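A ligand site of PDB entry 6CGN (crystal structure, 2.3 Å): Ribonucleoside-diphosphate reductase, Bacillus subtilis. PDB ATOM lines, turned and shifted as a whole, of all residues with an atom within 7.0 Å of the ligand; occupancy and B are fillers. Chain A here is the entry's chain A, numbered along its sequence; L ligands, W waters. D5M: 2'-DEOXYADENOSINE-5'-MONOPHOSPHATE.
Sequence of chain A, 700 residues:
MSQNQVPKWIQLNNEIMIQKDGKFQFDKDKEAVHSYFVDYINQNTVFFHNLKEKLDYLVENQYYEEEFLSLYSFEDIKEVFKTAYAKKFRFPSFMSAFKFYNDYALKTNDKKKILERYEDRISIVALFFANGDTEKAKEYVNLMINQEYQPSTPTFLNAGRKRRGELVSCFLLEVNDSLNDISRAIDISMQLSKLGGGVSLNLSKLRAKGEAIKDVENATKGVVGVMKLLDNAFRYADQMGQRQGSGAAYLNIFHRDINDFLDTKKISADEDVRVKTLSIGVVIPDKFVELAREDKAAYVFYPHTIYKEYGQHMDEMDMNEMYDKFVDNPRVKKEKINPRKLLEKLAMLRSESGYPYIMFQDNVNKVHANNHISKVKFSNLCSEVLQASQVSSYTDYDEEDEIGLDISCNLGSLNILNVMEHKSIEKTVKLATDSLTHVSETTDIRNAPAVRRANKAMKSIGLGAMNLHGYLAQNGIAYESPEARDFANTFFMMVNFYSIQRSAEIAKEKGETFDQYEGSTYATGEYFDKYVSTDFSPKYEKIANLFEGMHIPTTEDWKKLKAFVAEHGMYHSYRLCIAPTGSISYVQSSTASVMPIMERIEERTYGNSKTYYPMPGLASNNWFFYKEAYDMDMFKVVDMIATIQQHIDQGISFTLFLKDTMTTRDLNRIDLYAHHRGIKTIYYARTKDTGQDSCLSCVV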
ATOM      1  N   ASP A  29     -28.979   1.350  15.322  1.00  0.00           N
ATOM      2  CA  ASP A  29     -28.037   2.463  15.345  1.00  0.00           C
ATOM      3  C   ASP A  29     -28.559   3.668  14.530  1.00  0.00           C
ATOM      4  O   ASP A  29     -28.316   4.808  14.913  1.00  0.00           O
ATOM      5  CB  ASP A  29     -26.653   2.034  14.823  1.00  0.00           C
ATOM      6  CG  ASP A  29     -25.500   2.844  15.415  1.00  0.00           C
ATOM      7  OD1 ASP A  29     -24.395   2.790  14.843  1.00  0.00           O
ATOM      8  OD2 ASP A  29     -25.679   3.525  16.443  1.00  0.00           O
ATOM      9  N   LYS A  30     -29.265   3.389  13.436  1.00  0.00           N
ATOM     10  CA  LYS A  30     -29.889   4.436  12.608  1.00  0.00           C
ATOM     11  C   LYS A  30     -31.003   5.169  13.367  1.00  0.00           C
ATOM     12  O   LYS A  30     -31.149   6.392  13.248  1.00  0.00           O
ATOM     13  CB  LYS A  30     -30.450   3.868  11.294  1.00  0.00           C
ATOM     14  CG  LYS A  30     -29.427   3.209  10.384  1.00  0.00           C
ATOM     15  CD  LYS A  30     -28.592   4.214   9.610  1.00  0.00           C
ATOM     16  CE  LYS A  30     -27.426   3.555   8.891  1.00  0.00           C
ATOM     17  NZ  LYS A  30     -27.867   2.600   7.842  1.00  0.00           N
ATOM     18  N   VAL A  33     -29.137   7.387  16.231  1.00  0.00           N
ATOM     19  CA  VAL A  33     -28.638   8.658  15.711  1.00  0.00           C
ATOM     20  C   VAL A  33     -29.766   9.640  15.387  1.00  0.00           C
ATOM     21  O   VAL A  33     -29.643  10.824  15.663  1.00  0.00           O
ATOM     22  CB  VAL A  33     -27.653   8.488  14.507  1.00  0.00           C
ATOM     23  CG1 VAL A  33     -28.337   7.915  13.264  1.00  0.00           C
ATOM     24  CG2 VAL A  33     -26.951   9.793  14.183  1.00  0.00           C
ATOM     25  N   HIS A  34     -30.871   9.136  14.841  1.00  0.00           N
ATOM     26  CA  HIS A  34     -32.059   9.958  14.580  1.00  0.00           C
ATOM     27  C   HIS A  34     -32.595  10.589  15.871  1.00  0.00           C
ATOM     28  O   HIS A  34     -32.944  11.773  15.879  1.00  0.00           O
ATOM     29  CB  HIS A  34     -33.154   9.134  13.893  1.00  0.00           C
ATOM     30  CG  HIS A  34     -34.379   9.916  13.554  1.00  0.00           C
ATOM     31  ND1 HIS A  34     -35.453  10.017  14.401  1.00  0.00           N
ATOM     32  CD2 HIS A  34     -34.682  10.664  12.464  1.00  0.00           C
ATOM     33  CE1 HIS A  34     -36.380  10.781  13.841  1.00  0.00           C
ATOM     34  NE2 HIS A  34     -35.933  11.180  12.673  1.00  0.00           N
ATOM     35  N   SER A  35     -32.653   9.799  16.934  1.00  0.00           N
ATOM     36  CA  SER A  35     -33.050  10.281  18.264  1.00  0.00           C
ATOM     37  C   SER A  35     -32.080  11.332  18.797  1.00  0.00           C
ATOM     38  O   SER A  35     -32.497  12.353  19.327  1.00  0.00           O
ATOM     39  CB  SER A  35     -33.171   9.124  19.251  1.00  0.00           C
ATOM     40  OG  SER A  35     -33.468   9.592  20.563  1.00  0.00           O
ATOM     41  N   TYR A  36     -30.778  11.078  18.642  1.00  0.00           N
ATOM     42  CA  TYR A  36     -29.722  12.016  19.042  1.00  0.00           C
ATOM     43  C   TYR A  36     -29.904  13.412  18.429  1.00  0.00           C
ATOM     44  O   TYR A  36     -29.640  14.423  19.096  1.00  0.00           O
ATOM     45  CB  TYR A  36     -28.351  11.436  18.666  1.00  0.00           C
ATOM     46  CG  TYR A  36     -27.157  12.275  19.078  1.00  0.00           C
ATOM     47  CD1 TYR A  36     -26.944  12.617  20.418  1.00  0.00           C
ATOM     48  CD2 TYR A  36     -26.221  12.700  18.138  1.00  0.00           C
ATOM     49  CE1 TYR A  36     -25.837  13.372  20.794  1.00  0.00           C
ATOM     50  CE2 TYR A  36     -25.117  13.447  18.499  1.00  0.00           C
ATOM     51  CZ  TYR A  36     -24.928  13.778  19.823  1.00  0.00           C
ATOM     52  OH  TYR A  36     -23.825  14.525  20.184  1.00  0.00           O
ATOM     53  N   PHE A  37     -30.369  13.486  17.183  1.00  0.00           N
ATOM     54  CA  PHE A  37     -30.674  14.763  16.551  1.00  0.00           C
ATOM     55  C   PHE A  37     -32.001  15.365  17.037  1.00  0.00           C
ATOM     56  O   PHE A  37     -32.013  16.480  17.563  1.00  0.00           O
ATOM     57  CB  PHE A  37     -30.609  14.665  15.023  1.00  0.00           C
ATOM     58  CG  PHE A  37     -29.206  14.713  14.483  1.00  0.00           C
ATOM     59  CD1 PHE A  37     -28.604  15.931  14.197  1.00  0.00           C
ATOM     60  CD2 PHE A  37     -28.479  13.541  14.288  1.00  0.00           C
ATOM     61  CE1 PHE A  37     -27.301  15.975  13.704  1.00  0.00           C
ATOM     62  CE2 PHE A  37     -27.180  13.581  13.804  1.00  0.00           C
ATOM     63  CZ  PHE A  37     -26.587  14.798  13.514  1.00  0.00           C
ATOM     64  N   VAL A  38     -33.103  14.631  16.856  1.00  0.00           N
ATOM     65  CA  VAL A  38     -34.448  15.174  17.161  1.00  0.00           C
ATOM     66  C   VAL A  38     -34.765  15.327  18.667  1.00  0.00           C
ATOM     67  O   VAL A  38     -35.697  16.050  19.005  1.00  0.00           O
ATOM     68  CB  VAL A  38     -35.590  14.372  16.473  1.00  0.00           C
ATOM     69  CG1 VAL A  38     -35.347  14.298  14.964  1.00  0.00           C
ATOM     70  CG2 VAL A  38     -35.763  12.980  17.080  1.00  0.00           C
ATOM     71  N   ASN A  42     -30.830  19.027  17.755  1.00  0.00           N
ATOM     72  CA  ASN A  42     -31.750  20.020  17.181  1.00  0.00           C
ATOM     73  C   ASN A  42     -32.422  20.927  18.214  1.00  0.00           C
ATOM     74  O   ASN A  42     -32.951  21.979  17.860  1.00  0.00           O
ATOM     75  CB  ASN A  42     -32.834  19.330  16.329  1.00  0.00           C
ATOM     76  CG  ASN A  42     -32.254  18.565  15.134  1.00  0.00           C
ATOM     77  OD1 ASN A  42     -31.081  18.734  14.771  1.00  0.00           O
ATOM     78  ND2 ASN A  42     -33.065  17.719  14.530  1.00  0.00           N
ATOM     79  N   LYS A  88     -27.950  16.462   1.447  1.00  0.00           N
ATOM     80  CA  LYS A  88     -28.706  15.710   2.446  1.00  0.00           C
ATOM     81  C   LYS A  88     -27.823  14.734   3.231  1.00  0.00           C
ATOM     82  O   LYS A  88     -28.131  13.533   3.318  1.00  0.00           O
ATOM     83  CB  LYS A  88     -29.879  14.944   1.792  1.00  0.00           C
ATOM     84  CG  LYS A  88     -30.901  15.824   1.083  1.00  0.00           C
ATOM     85  CD  LYS A  88     -31.729  16.674   2.037  1.00  0.00           C
ATOM     86  CE  LYS A  88     -32.618  15.824   2.938  1.00  0.00           C
ATOM     87  NZ  LYS A  88     -33.604  16.641   3.694  1.00  0.00           N
ATOM     88  N   PHE A  89     -26.722  15.235   3.785  1.00  0.00           N
ATOM     89  CA  PHE A  89     -25.789  14.383   4.512  1.00  0.00           C
ATOM     90  C   PHE A  89     -26.416  13.867   5.799  1.00  0.00           C
ATOM     91  O   PHE A  89     -26.920  14.643   6.602  1.00  0.00           O
ATOM     92  CB  PHE A  89     -24.475  15.093   4.836  1.00  0.00           C
ATOM     93  CG  PHE A  89     -23.476  14.192   5.528  1.00  0.00           C
ATOM     94  CD1 PHE A  89     -23.382  14.176   6.909  1.00  0.00           C
ATOM     95  CD2 PHE A  89     -22.691  13.314   4.787  1.00  0.00           C
ATOM     96  CE1 PHE A  89     -22.485  13.319   7.549  1.00  0.00           C
ATOM     97  CE2 PHE A  89     -21.797  12.472   5.408  1.00  0.00           C
ATOM     98  CZ  PHE A  89     -21.684  12.471   6.792  1.00  0.00           C
ATOM     99  N   ARG A  90     -26.371  12.548   5.986  1.00  0.00           N
ATOM    100  CA  ARG A  90     -26.859  11.906   7.193  1.00  0.00           C
ATOM    101  C   ARG A  90     -25.782  10.986   7.750  1.00  0.00           C
ATOM    102  O   ARG A  90     -25.152  10.222   7.007  1.00  0.00           O
ATOM    103  CB  ARG A  90     -28.150  11.116   6.907  1.00  0.00           C
ATOM    104  CG  ARG A  90     -29.353  11.983   6.552  1.00  0.00           C
ATOM    105  CD  ARG A  90     -29.888  12.730   7.772  1.00  0.00           C
ATOM    106  NE  ARG A  90     -30.999  13.640   7.451  1.00  0.00           N
ATOM    107  CZ  ARG A  90     -30.876  14.827   6.847  1.00  0.00           C
ATOM    108  NH1 ARG A  90     -29.692  15.311   6.469  1.00  0.00           N
ATOM    109  NH2 ARG A  90     -31.969  15.556   6.616  1.00  0.00           N
ATOM    110  N   PHE A  91     -25.542  11.076   9.062  1.00  0.00           N
ATOM    111  CA  PHE A  91     -24.624  10.187   9.757  1.00  0.00           C
ATOM    112  C   PHE A  91     -25.260   8.798   9.869  1.00  0.00           C
ATOM    113  O   PHE A  91     -26.417   8.698  10.302  1.00  0.00           O
ATOM    114  CB  PHE A  91     -24.291  10.732  11.158  1.00  0.00           C
ATOM    115  CG  PHE A  91     -23.388  11.936  11.129  1.00  0.00           C
ATOM    116  CD1 PHE A  91     -23.917  13.225  11.259  1.00  0.00           C
ATOM    117  CD2 PHE A  91     -22.017  11.783  10.973  1.00  0.00           C
ATOM    118  CE1 PHE A  91     -23.079  14.336  11.246  1.00  0.00           C
ATOM    119  CE2 PHE A  91     -21.176  12.897  10.951  1.00  0.00           C
ATOM    120  CZ  PHE A  91     -21.716  14.172  11.083  1.00  0.00           C
ATOM    121  N   PRO A  92     -24.529   7.733   9.485  1.00  0.00           N
ATOM    122  CA  PRO A  92     -25.095   6.374   9.583  1.00  0.00           C
ATOM    123  C   PRO A  92     -25.081   5.768  10.992  1.00  0.00           C
ATOM    124  O   PRO A  92     -25.757   4.771  11.225  1.00  0.00           O
ATOM    125  CB  PRO A  92     -24.184   5.566   8.658  1.00  0.00           C
ATOM    126  CG  PRO A  92     -22.864   6.252   8.767  1.00  0.00           C
ATOM    127  CD  PRO A  92     -23.153   7.715   8.967  1.00  0.00           C
ATOM    128  N   SER A  93     -24.339   6.368  11.924  1.00  0.00           N
ATOM    129  CA  SER A  93     -24.190   5.832  13.269  1.00  0.00           C
ATOM    130  C   SER A  93     -24.296   6.929  14.315  1.00  0.00           C
ATOM    131  O   SER A  93     -24.088   8.107  14.001  1.00  0.00           O
ATOM    132  CB  SER A  93     -22.825   5.159  13.411  1.00  0.00           C
ATOM    133  OG  SER A  93     -21.804   6.071  13.078  1.00  0.00           O
ATOM    134  N   ALA A  97     -21.873  10.835  14.467  1.00  0.00           N
ATOM    135  CA  ALA A  97     -22.522  12.108  14.781  1.00  0.00           C
ATOM    136  C   ALA A  97     -22.057  12.653  16.137  1.00  0.00           C
ATOM    137  O   ALA A  97     -21.759  13.836  16.259  1.00  0.00           O
ATOM    138  CB  ALA A  97     -24.029  11.957  14.771  1.00  0.00           C
ATOM    139  N   TYR A 101     -20.131  16.402  16.819  1.00  0.00           N
ATOM    140  CA  TYR A 101     -20.781  17.455  17.617  1.00  0.00           C
ATOM    141  C   TYR A 101     -20.176  17.650  19.005  1.00  0.00           C
ATOM    142  O   TYR A 101     -20.295  18.729  19.574  1.00  0.00           O
ATOM    143  CB  TYR A 101     -22.303  17.231  17.699  1.00  0.00           C
ATOM    144  CG  TYR A 101     -22.982  17.638  16.416  1.00  0.00           C
ATOM    145  CD1 TYR A 101     -23.372  16.699  15.465  1.00  0.00           C
ATOM    146  CD2 TYR A 101     -23.204  18.988  16.127  1.00  0.00           C
ATOM    147  CE1 TYR A 101     -23.967  17.080  14.267  1.00  0.00           C
ATOM    148  CE2 TYR A 101     -23.794  19.389  14.939  1.00  0.00           C
ATOM    149  CZ  TYR A 101     -24.175  18.432  14.020  1.00  0.00           C
ATOM    150  OH  TYR A 101     -24.771  18.817  12.846  1.00  0.00           O
ATOM    151  N   ARG A 117     -23.686  23.359  12.367  1.00  0.00           N
ATOM    152  CA  ARG A 117     -24.000  22.024  11.867  1.00  0.00           C
ATOM    153  C   ARG A 117     -22.714  21.500  11.219  1.00  0.00           C
ATOM    154  O   ARG A 117     -21.752  22.252  10.995  1.00  0.00           O
ATOM    155  CB  ARG A 117     -25.120  22.031  10.814  1.00  0.00           C
ATOM    156  CG  ARG A 117     -26.370  22.860  11.120  1.00  0.00           C
ATOM    157  CD  ARG A 117     -27.212  22.327  12.257  1.00  0.00           C
ATOM    158  NE  ARG A 117     -27.829  21.034  11.962  1.00  0.00           N
ATOM    159  CZ  ARG A 117     -28.839  20.495  12.640  1.00  0.00           C
ATOM    160  NH1 ARG A 117     -29.425  21.126  13.664  1.00  0.00           N
ATOM    161  NH2 ARG A 117     -29.308  19.299  12.274  1.00  0.00           N
ATOM    162  N   GLU A 119     -22.416  20.816   8.143  1.00  0.00           N
ATOM    163  CA  GLU A 119     -22.338  21.521   6.871  1.00  0.00           C
ATOM    164  C   GLU A 119     -21.734  22.930   7.007  1.00  0.00           C
ATOM    165  O   GLU A 119     -21.118  23.430   6.069  1.00  0.00           O
ATOM    166  CB  GLU A 119     -23.728  21.603   6.202  1.00  0.00           C
ATOM    167  CG  GLU A 119     -24.290  20.273   5.709  1.00  0.00           C
ATOM    168  CD  GLU A 119     -25.026  19.454   6.772  1.00  0.00           C
ATOM    169  OE1 GLU A 119     -24.888  19.731   7.983  1.00  0.00           O
ATOM    170  OE2 GLU A 119     -25.753  18.503   6.385  1.00  0.00           O
HETATM  171  O5' D5M L   1     -33.810  14.646   9.831  1.00  0.00           O
HETATM  172  C5' D5M L   1     -34.524  15.678  10.535  1.00  0.00           C
HETATM  173  C4' D5M L   1     -33.564  16.608  11.226  1.00  0.00           C
HETATM  174  O4' D5M L   1     -32.706  15.842  12.116  1.00  0.00           O
HETATM  175  C3' D5M L   1     -32.622  17.370  10.302  1.00  0.00           C
HETATM  176  O3' D5M L   1     -32.302  18.653  10.844  1.00  0.00           O
HETATM  177  C2' D5M L   1     -31.397  16.487  10.243  1.00  0.00           C
HETATM  178  C1' D5M L   1     -31.381  15.791  11.596  1.00  0.00           C
HETATM  179  N9  D5M L   1     -30.982  14.386  11.549  1.00  0.00           N
HETATM  180  C8  D5M L   1     -31.716  13.265  11.836  1.00  0.00           C
HETATM  181  N7  D5M L   1     -31.056  12.145  11.701  1.00  0.00           N
HETATM  182  C5  D5M L   1     -29.796  12.555  11.271  1.00  0.00           C
HETATM  183  C6  D5M L   1     -28.627  11.839  10.949  1.00  0.00           C
HETATM  184  N6  D5M L   1     -28.534  10.508  10.991  1.00  0.00           N
HETATM  185  N1  D5M L   1     -27.541  12.546  10.567  1.00  0.00           N
HETATM  186  C2  D5M L   1     -27.639  13.879  10.512  1.00  0.00           C
HETATM  187  N3  D5M L   1     -28.674  14.669  10.795  1.00  0.00           N
HETATM  188  C4  D5M L   1     -29.734  13.926  11.175  1.00  0.00           C
HETATM  189  P   D5M L   1     -34.567  13.584   8.902  1.00  0.00           P
HETATM  190  O1P D5M L   1     -33.540  12.872   8.112  1.00  0.00           O
HETATM  191  O3P D5M L   1     -35.153  12.614   9.870  1.00  0.00           O
HETATM  192  O2P D5M L   1     -35.692  14.275   8.213  1.00  0.00           O
HETATM  193  O   HOH W   1     -27.984  17.447  10.786  1.00  0.00           O
HETATM  194  O   HOH W   2     -36.504  10.145   8.508  1.00  0.00           O
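A nitrogen (N6) of the ligand is in hydrogen-bond range of the backbone carbonyl oxygen (O) of Phe 91, 2.9 Å away. The side-chain amide nitrogen (ND2) of Asn 42 lies within hydrogen-bond range of an oxygen (O4') of the ligand, at 3.1 Å. O3P of the ligand lies within hydrogen-bond range of NE2 of His 34. An oxygen (O1P) of the ligand is in salt-bridge range of the guanidinium group (NE) of Arg 90 (2.7 Å). A nitrogen (N1) of the ligand is in hydrogen-bond range of the backbone NH (N) of Phe 91 (2.9 Å). The guanidinium group (NH2) of Arg 117 lies within hydrogen-bond range of an oxygen (O3') of the ligand, 3.4 Å away.
N of Asn 42 lies within hydrogen-bond range of O of Phe 37 (2.8 Å). NH1 of Arg 117 lies within hydrogen-bond range of OD1 of Asn 42, at 3.1 Å.
Val 33 touches the ligand (CG1 to N6, 3.5 Å). Phe 37 touches the ligand (CZ to C2, 3.3 Å). Hydrophobic or aromatic side chains within 4 Å of the ligand: Val 33, His 34, Phe 37 and Phe 91. Of the 19 residues printed, 7 come within 4 Å of the ligand. The nearest printed residue that does not touch the ligand is Phe 89 (4.05 Å).
Water W1 bridges NH2 of Arg 117 and N3 of the ligand.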
